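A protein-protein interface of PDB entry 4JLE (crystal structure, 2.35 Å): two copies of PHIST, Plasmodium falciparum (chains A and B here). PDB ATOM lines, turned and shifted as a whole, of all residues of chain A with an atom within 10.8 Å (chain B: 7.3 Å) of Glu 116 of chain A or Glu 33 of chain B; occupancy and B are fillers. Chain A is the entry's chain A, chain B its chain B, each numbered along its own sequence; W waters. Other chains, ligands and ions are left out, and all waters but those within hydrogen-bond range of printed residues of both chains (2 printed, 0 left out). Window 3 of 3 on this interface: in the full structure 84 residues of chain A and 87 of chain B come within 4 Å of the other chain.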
ATOM      1  N   ASN A 111       0.089   4.437  17.475  1.00  0.00           N
ATOM      2  CA  ASN A 111      -0.994   4.045  16.554  1.00  0.00           C
ATOM      3  C   ASN A 111      -1.717   2.800  17.152  1.00  0.00           C
ATOM      4  O   ASN A 111      -1.052   1.966  17.789  1.00  0.00           O
ATOM      5  CB  ASN A 111      -0.442   3.800  15.119  1.00  0.00           C
ATOM      6  CG  ASN A 111      -1.472   3.630  14.002  1.00  0.00           C
ATOM      7  OD1 ASN A 111      -2.480   4.343  13.904  1.00  0.00           O
ATOM      8  ND2 ASN A 111      -1.220   2.698  13.087  1.00  0.00           N
ATOM      9  N   GLY A 112      -3.062   2.753  17.027  1.00  0.00           N
ATOM     10  CA  GLY A 112      -3.907   1.712  17.597  1.00  0.00           C
ATOM     11  C   GLY A 112      -3.799   0.386  16.896  1.00  0.00           C
ATOM     12  O   GLY A 112      -3.427   0.352  15.721  1.00  0.00           O
ATOM     13  N   LYS A 113      -4.138  -0.713  17.612  1.00  0.00           N
ATOM     14  CA  LYS A 113      -4.095  -2.090  17.114  1.00  0.00           C
ATOM     15  C   LYS A 113      -5.009  -2.329  15.895  1.00  0.00           C
ATOM     16  O   LYS A 113      -4.675  -3.183  15.076  1.00  0.00           O
ATOM     17  CB  LYS A 113      -4.446  -3.118  18.218  1.00  0.00           C
ATOM     18  CG  LYS A 113      -3.424  -3.206  19.370  1.00  0.00           C
ATOM     19  CD  LYS A 113      -2.272  -4.190  19.104  1.00  0.00           C
ATOM     20  CE  LYS A 113      -1.155  -4.058  20.114  1.00  0.00           C
ATOM     21  NZ  LYS A 113       0.110  -4.664  19.620  1.00  0.00           N
ATOM     22  N   LEU A 114      -6.155  -1.627  15.800  1.00  0.00           N
ATOM     23  CA  LEU A 114      -7.096  -1.790  14.681  1.00  0.00           C
ATOM     24  C   LEU A 114      -7.532  -0.479  14.069  1.00  0.00           C
ATOM     25  O   LEU A 114      -7.639   0.523  14.768  1.00  0.00           O
ATOM     26  CB  LEU A 114      -8.375  -2.521  15.122  1.00  0.00           C
ATOM     27  CG  LEU A 114      -8.324  -3.992  15.385  1.00  0.00           C
ATOM     28  CD1 LEU A 114      -9.631  -4.448  16.066  1.00  0.00           C
ATOM     29  CD2 LEU A 114      -8.064  -4.774  14.070  1.00  0.00           C
ATOM     30  N   CYS A 115      -7.890  -0.514  12.791  1.00  0.00           N
ATOM     31  CA  CYS A 115      -8.397   0.636  12.068  1.00  0.00           C
ATOM     32  C   CYS A 115      -9.346   0.167  10.970  1.00  0.00           C
ATOM     33  O   CYS A 115      -9.158  -0.910  10.400  1.00  0.00           O
ATOM     34  CB  CYS A 115      -7.244   1.466  11.502  1.00  0.00           C
ATOM     35  SG  CYS A 115      -7.774   2.949  10.620  1.00  0.00           S
ATOM     36  N   GLU A 116     -10.345   0.980  10.643  1.00  0.00           N
ATOM     37  CA  GLU A 116     -11.243   0.708   9.513  1.00  0.00           C
ATOM     38  C   GLU A 116     -10.399   0.714   8.229  1.00  0.00           C
ATOM     39  O   GLU A 116      -9.687   1.690   7.987  1.00  0.00           O
ATOM     40  CB  GLU A 116     -12.382   1.756   9.447  1.00  0.00           C
ATOM     41  CG  GLU A 116     -13.591   1.279   8.666  1.00  0.00           C
ATOM     42  CD  GLU A 116     -14.558   2.317   8.120  1.00  0.00           C
ATOM     43  OE1 GLU A 116     -14.203   3.519   8.066  1.00  0.00           O
ATOM     44  OE2 GLU A 116     -15.671   1.911   7.709  1.00  0.00           O
ATOM     45  N   ARG A 117     -10.419  -0.375   7.457  1.00  0.00           N
ATOM     46  CA  ARG A 117      -9.608  -0.483   6.231  1.00  0.00           C
ATOM     47  C   ARG A 117      -9.887   0.657   5.222  1.00  0.00           C
ATOM     48  O   ARG A 117      -8.958   1.127   4.577  1.00  0.00           O
ATOM     49  CB  ARG A 117      -9.812  -1.848   5.554  1.00  0.00           C
ATOM     50  CG  ARG A 117      -8.638  -2.229   4.628  1.00  0.00           C
ATOM     51  CD  ARG A 117      -8.768  -3.637   4.071  1.00  0.00           C
ATOM     52  NE  ARG A 117      -8.622  -4.643   5.123  1.00  0.00           N
ATOM     53  CZ  ARG A 117      -7.508  -5.314   5.368  1.00  0.00           C
ATOM     54  NH1 ARG A 117      -6.442  -5.139   4.606  1.00  0.00           N
ATOM     55  NH2 ARG A 117      -7.457  -6.180   6.368  1.00  0.00           N
ATOM     56  N   LYS A 118     -11.155   1.089   5.100  1.00  0.00           N
ATOM     57  CA  LYS A 118     -11.630   2.169   4.214  1.00  0.00           C
ATOM     58  C   LYS A 118     -10.830   3.460   4.475  1.00  0.00           C
ATOM     59  O   LYS A 118     -10.273   4.040   3.540  1.00  0.00           O
ATOM     60  CB  LYS A 118     -13.147   2.404   4.454  1.00  0.00           C
ATOM     61  CG  LYS A 118     -13.862   3.236   3.389  1.00  0.00           C
ATOM     62  CD  LYS A 118     -15.026   4.014   3.993  1.00  0.00           C
ATOM     63  CE  LYS A 118     -15.724   4.911   3.000  1.00  0.00           C
ATOM     64  NZ  LYS A 118     -16.652   4.154   2.115  1.00  0.00           N
ATOM     65  N   LYS A 119     -10.778   3.877   5.755  1.00  0.00           N
ATOM     66  CA  LYS A 119     -10.068   5.035   6.273  1.00  0.00           C
ATOM     67  C   LYS A 119      -8.546   4.901   6.026  1.00  0.00           C
ATOM     68  O   LYS A 119      -7.894   5.878   5.671  1.00  0.00           O
ATOM     69  CB  LYS A 119     -10.358   5.162   7.781  1.00  0.00           C
ATOM     70  CG  LYS A 119      -9.812   6.425   8.448  1.00  0.00           C
ATOM     71  CD  LYS A 119      -9.688   6.225   9.965  1.00  0.00           C
ATOM     72  CE  LYS A 119     -10.872   6.699  10.787  1.00  0.00           C
ATOM     73  NZ  LYS A 119     -10.553   6.733  12.244  1.00  0.00           N
ATOM     74  N   PHE A 120      -7.978   3.701   6.269  1.00  0.00           N
ATOM     75  CA  PHE A 120      -6.561   3.429   6.051  1.00  0.00           C
ATOM     76  C   PHE A 120      -6.213   3.627   4.563  1.00  0.00           C
ATOM     77  O   PHE A 120      -5.209   4.251   4.264  1.00  0.00           O
ATOM     78  CB  PHE A 120      -6.196   2.012   6.515  1.00  0.00           C
ATOM     79  CG  PHE A 120      -4.761   1.660   6.218  1.00  0.00           C
ATOM     80  CD1 PHE A 120      -3.727   2.170   7.000  1.00  0.00           C
ATOM     81  CD2 PHE A 120      -4.439   0.853   5.136  1.00  0.00           C
ATOM     82  CE1 PHE A 120      -2.390   1.877   6.700  1.00  0.00           C
ATOM     83  CE2 PHE A 120      -3.107   0.548   4.845  1.00  0.00           C
ATOM     84  CZ  PHE A 120      -2.091   1.053   5.635  1.00  0.00           C
ATOM     85  N   LYS A 121      -7.046   3.107   3.658  1.00  0.00           N
ATOM     86  CA  LYS A 121      -6.928   3.198   2.215  1.00  0.00           C
ATOM     87  C   LYS A 121      -6.997   4.668   1.764  1.00  0.00           C
ATOM     88  O   LYS A 121      -6.216   5.079   0.904  1.00  0.00           O
ATOM     89  CB  LYS A 121      -8.052   2.354   1.579  1.00  0.00           C
ATOM     90  CG  LYS A 121      -7.884   2.037   0.113  1.00  0.00           C
ATOM     91  CD  LYS A 121      -8.936   1.057  -0.379  1.00  0.00           C
ATOM     92  CE  LYS A 121      -9.377   1.389  -1.788  1.00  0.00           C
ATOM     93  NZ  LYS A 121      -8.324   1.142  -2.820  1.00  0.00           N
ATOM     94  N   GLU A 122      -7.892   5.466   2.381  1.00  0.00           N
ATOM     95  CA  GLU A 122      -8.028   6.889   2.092  1.00  0.00           C
ATOM     96  C   GLU A 122      -6.740   7.641   2.455  1.00  0.00           C
ATOM     97  O   GLU A 122      -6.234   8.429   1.649  1.00  0.00           O
ATOM     98  CB  GLU A 122      -9.217   7.491   2.863  1.00  0.00           C
ATOM     99  CG  GLU A 122     -10.581   7.167   2.279  1.00  0.00           C
ATOM    100  CD  GLU A 122     -11.782   7.472   3.158  1.00  0.00           C
ATOM    101  OE1 GLU A 122     -11.656   8.327   4.066  1.00  0.00           O
ATOM    102  OE2 GLU A 122     -12.861   6.880   2.914  1.00  0.00           O
ATOM    103  N   VAL A 123      -6.210   7.405   3.677  1.00  0.00           N
ATOM    104  CA  VAL A 123      -4.981   8.026   4.178  1.00  0.00           C
ATOM    105  C   VAL A 123      -3.821   7.669   3.237  1.00  0.00           C
ATOM    106  O   VAL A 123      -3.063   8.546   2.847  1.00  0.00           O
ATOM    107  CB  VAL A 123      -4.690   7.591   5.644  1.00  0.00           C
ATOM    108  CG1 VAL A 123      -3.272   7.949   6.087  1.00  0.00           C
ATOM    109  CG2 VAL A 123      -5.704   8.187   6.593  1.00  0.00           C
ATOM    110  N   LEU A 124      -3.715   6.387   2.869  1.00  0.00           N
ATOM    111  CA  LEU A 124      -2.692   5.841   1.990  1.00  0.00           C
ATOM    112  C   LEU A 124      -2.746   6.477   0.604  1.00  0.00           C
ATOM    113  O   LEU A 124      -1.710   6.813   0.073  1.00  0.00           O
ATOM    114  CB  LEU A 124      -2.883   4.327   1.898  1.00  0.00           C
ATOM    115  CG  LEU A 124      -1.698   3.506   1.463  1.00  0.00           C
ATOM    116  CD1 LEU A 124      -0.530   3.567   2.488  1.00  0.00           C
ATOM    117  CD2 LEU A 124      -2.138   2.083   1.281  1.00  0.00           C
ATOM    118  N   SER B  30      -8.331  -5.439   0.242  1.00  0.00           N
ATOM    119  CA  SER B  30      -9.026  -6.513   0.948  1.00  0.00           C
ATOM    120  C   SER B  30     -10.458  -6.106   1.291  1.00  0.00           C
ATOM    121  O   SER B  30     -10.724  -4.928   1.602  1.00  0.00           O
ATOM    122  CB  SER B  30      -8.267  -6.894   2.215  1.00  0.00           C
ATOM    123  OG  SER B  30      -8.975  -7.864   2.967  1.00  0.00           O
ATOM    124  N   SER B  31     -11.383  -7.081   1.227  1.00  0.00           N
ATOM    125  CA  SER B  31     -12.803  -6.854   1.534  1.00  0.00           C
ATOM    126  C   SER B  31     -13.014  -6.698   3.049  1.00  0.00           C
ATOM    127  O   SER B  31     -14.007  -6.092   3.455  1.00  0.00           O
ATOM    128  CB  SER B  31     -13.683  -7.966   0.963  1.00  0.00           C
ATOM    129  OG  SER B  31     -13.210  -9.242   1.364  1.00  0.00           O
ATOM    130  N   ASN B  32     -12.059  -7.198   3.876  1.00  0.00           N
ATOM    131  CA  ASN B  32     -12.066  -7.088   5.351  1.00  0.00           C
ATOM    132  C   ASN B  32     -12.310  -5.636   5.806  1.00  0.00           C
ATOM    133  O   ASN B  32     -11.626  -4.719   5.320  1.00  0.00           O
ATOM    134  CB  ASN B  32     -10.739  -7.606   5.925  1.00  0.00           C
ATOM    135  CG  ASN B  32     -10.551  -9.081   5.706  1.00  0.00           C
ATOM    136  OD1 ASN B  32     -10.924  -9.640   4.676  1.00  0.00           O
ATOM    137  ND2 ASN B  32      -9.983  -9.751   6.678  1.00  0.00           N
ATOM    138  N   GLU B  33     -13.312  -5.428   6.696  1.00  0.00           N
ATOM    139  CA  GLU B  33     -13.672  -4.093   7.158  1.00  0.00           C
ATOM    140  C   GLU B  33     -12.567  -3.402   7.955  1.00  0.00           C
ATOM    141  O   GLU B  33     -12.453  -2.171   7.929  1.00  0.00           O
ATOM    142  CB  GLU B  33     -14.954  -4.111   8.014  1.00  0.00           C
ATOM    143  CG  GLU B  33     -15.900  -3.002   7.585  1.00  0.00           C
ATOM    144  CD  GLU B  33     -16.635  -2.269   8.678  1.00  0.00           C
ATOM    145  OE1 GLU B  33     -17.656  -2.811   9.153  1.00  0.00           O
ATOM    146  OE2 GLU B  33     -16.206  -1.152   9.054  1.00  0.00           O
ATOM    147  N   PHE B  34     -11.817  -4.188   8.714  1.00  0.00           N
ATOM    148  CA  PHE B  34     -10.782  -3.662   9.560  1.00  0.00           C
ATOM    149  C   PHE B  34      -9.440  -4.174   9.126  1.00  0.00           C
ATOM    150  O   PHE B  34      -9.358  -5.214   8.485  1.00  0.00           O
ATOM    151  CB  PHE B  34     -11.055  -4.000  11.044  1.00  0.00           C
ATOM    152  CG  PHE B  34     -12.403  -3.523  11.543  1.00  0.00           C
ATOM    153  CD1 PHE B  34     -12.567  -2.238  12.031  1.00  0.00           C
ATOM    154  CD2 PHE B  34     -13.518  -4.356  11.487  1.00  0.00           C
ATOM    155  CE1 PHE B  34     -13.825  -1.787  12.452  1.00  0.00           C
ATOM    156  CE2 PHE B  34     -14.768  -3.904  11.909  1.00  0.00           C
ATOM    157  CZ  PHE B  34     -14.916  -2.623  12.381  1.00  0.00           C
ATOM    158  N   ILE B  35      -8.387  -3.410   9.467  1.00  0.00           N
ATOM    159  CA  ILE B  35      -6.997  -3.724   9.205  1.00  0.00           C
ATOM    160  C   ILE B  35      -6.255  -3.546  10.538  1.00  0.00           C
ATOM    161  O   ILE B  35      -6.445  -2.533  11.236  1.00  0.00           O
ATOM    162  CB  ILE B  35      -6.390  -2.905   8.018  1.00  0.00           C
ATOM    163  CG1 ILE B  35      -4.968  -3.432   7.636  1.00  0.00           C
ATOM    164  CG2 ILE B  35      -6.448  -1.360   8.226  1.00  0.00           C
ATOM    165  CD1 ILE B  35      -4.421  -2.888   6.259  1.00  0.00           C
ATOM    166  N   MET B  40      -0.787  -2.801   8.725  1.00  0.00           N
ATOM    167  CA  MET B  40      -0.565  -1.360   8.519  1.00  0.00           C
ATOM    168  C   MET B  40       0.917  -1.048   8.501  1.00  0.00           C
ATOM    169  O   MET B  40       1.367  -0.258   7.670  1.00  0.00           O
ATOM    170  CB  MET B  40      -1.265  -0.529   9.611  1.00  0.00           C
ATOM    171  CG  MET B  40      -2.822  -0.597   9.536  1.00  0.00           C
ATOM    172  SD  MET B  40      -3.557   0.640  10.653  1.00  0.00           S
ATOM    173  CE  MET B  40      -3.935  -0.369  12.155  1.00  0.00           C
ATOM    174  N   LEU B 110      -5.952   8.140  11.626  1.00  0.00           N
ATOM    175  CA  LEU B 110      -6.171   6.719  11.908  1.00  0.00           C
ATOM    176  C   LEU B 110      -6.463   6.415  13.370  1.00  0.00           C
ATOM    177  O   LEU B 110      -6.736   5.268  13.719  1.00  0.00           O
ATOM    178  CB  LEU B 110      -4.934   5.895  11.439  1.00  0.00           C
ATOM    179  CG  LEU B 110      -4.602   5.917   9.929  1.00  0.00           C
ATOM    180  CD1 LEU B 110      -3.303   5.259   9.678  1.00  0.00           C
ATOM    181  CD2 LEU B 110      -5.657   5.238   9.091  1.00  0.00           C
HETATM  182  O   HOH W   1      -9.836   4.129  12.697  1.00  0.00           O
HETATM  183  O   HOH W   2     -13.661  -0.432   6.019  1.00  0.00           O
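OE2 of Glu 116 of chain A sits close to OE2 of Glu 33 of chain B.
The guanidinium group of Arg 117 of chain A sits at hydrogen-bond distance from the backbone carbonyl oxygen of Phe 34 of chain B.
The backbone carbonyl oxygen (O) of Cys 115 of chain A lies within hydrogen-bond range of the backbone NH (N) of Ile 35 of chain B (2.8 Å).
The backbone carbonyl oxygen of Glu 33 of chain B is in hydrogen-bond range of the backbone NH of Arg 117 of chain A (2.8 Å).
O of Asn 32 of chain B sits at hydrogen-bond distance from NE of Arg 117 of chain A.
The side-chain hydroxyl (OG) of Ser 30 of chain B is in hydrogen-bond range of the side-chain amide oxygen (OD1) of Asn 32 of chain B, at 3.1 Å.
Among the printed residues, pairs that only touch across the chains: Cys 115 of chain A with Phe 34 of chain B (3.3 Å), Arg 117 of chain A with Ser 30 of chain B (3.4 Å), Arg 117 of chain A with Ile 35 of chain B (3.4 Å), Cys 115 of chain A with Leu 110 of chain B (3.5 Å), Leu 114 of chain A with Ile 35 of chain B (3.6 Å), Phe 120 of chain A with Leu 110 of chain B (3.7 Å), Gly 112 of chain A with Met 40 of chain B (3.7 Å), Phe 120 of chain A with Met 40 of chain B (3.8 Å), Phe 120 of chain A with Ile 35 of chain B (3.8 Å), Asn 111 of chain A with Leu 110 of chain B (3.8 Å), Cys 115 of chain A with Met 40 of chain B (3.8 Å), Val 123 of chain A with Leu 110 of chain B (3.9 Å) and Asn 111 of chain A with Met 40 of chain B (3.95 Å).
Of the printed residues of chain B, Asn 111 of chain A touches Met 40 (3.95 Å) and Leu 110 (3.8 Å).
Of the printed residues of chain B, Cys 115 of chain A touches Phe 34 (3.3 Å), Ile 35 (2.8 Å), Met 40 (3.8 Å) and Leu 110 (3.5 Å).
Of the printed residues of chain B, Glu 116 of chain A touches Glu 33.
No residue of chain A comes within 4 Å of Ser 31 of chain B.
Of chain A, only Cys 115 and Arg 117 come within 4 Å of Phe 34 of chain B.
Of the printed residues of chain A, Ile 35 of chain B touches Leu 114, Cys 115, Arg 117 and Phe 120.
Printed residues of chain A within 4 Å of Leu 110 of chain B: Asn 111, Cys 115, Phe 120 and Val 123.
The nearest printed residue of chain B that does not touch Leu 114 of chain A is Met 40 of chain B (4.1 Å).
Of the 14 printed residues of chain A, 8 touch a printed residue of chain B.
Hydrophobic or aromatic side chains of chain A within 4 Å of the printed part of chain B: Leu 114, Phe 120 and Val 123.
Hydrophobic or aromatic side chains of chain B within 4 Å of the printed part of chain A: Phe 34, Ile 35, Met 40 and Leu 110.
No position is printed for both chains.
Water W1 lies within hydrogen-bond range of the side-chain amino group of Lys 119 of chain A (2.7 Å), the side-chain sulfur of Cys 115 of chain A (3.2 Å) and the backbone carbonyl oxygen of Leu 110 of chain B (3.5 Å).
Water W2 bridges the backbone carbonyl oxygen of Glu 33 of chain B (2.9 Å) and the backbone NH of Lys 118 of chain A (3.1 Å).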
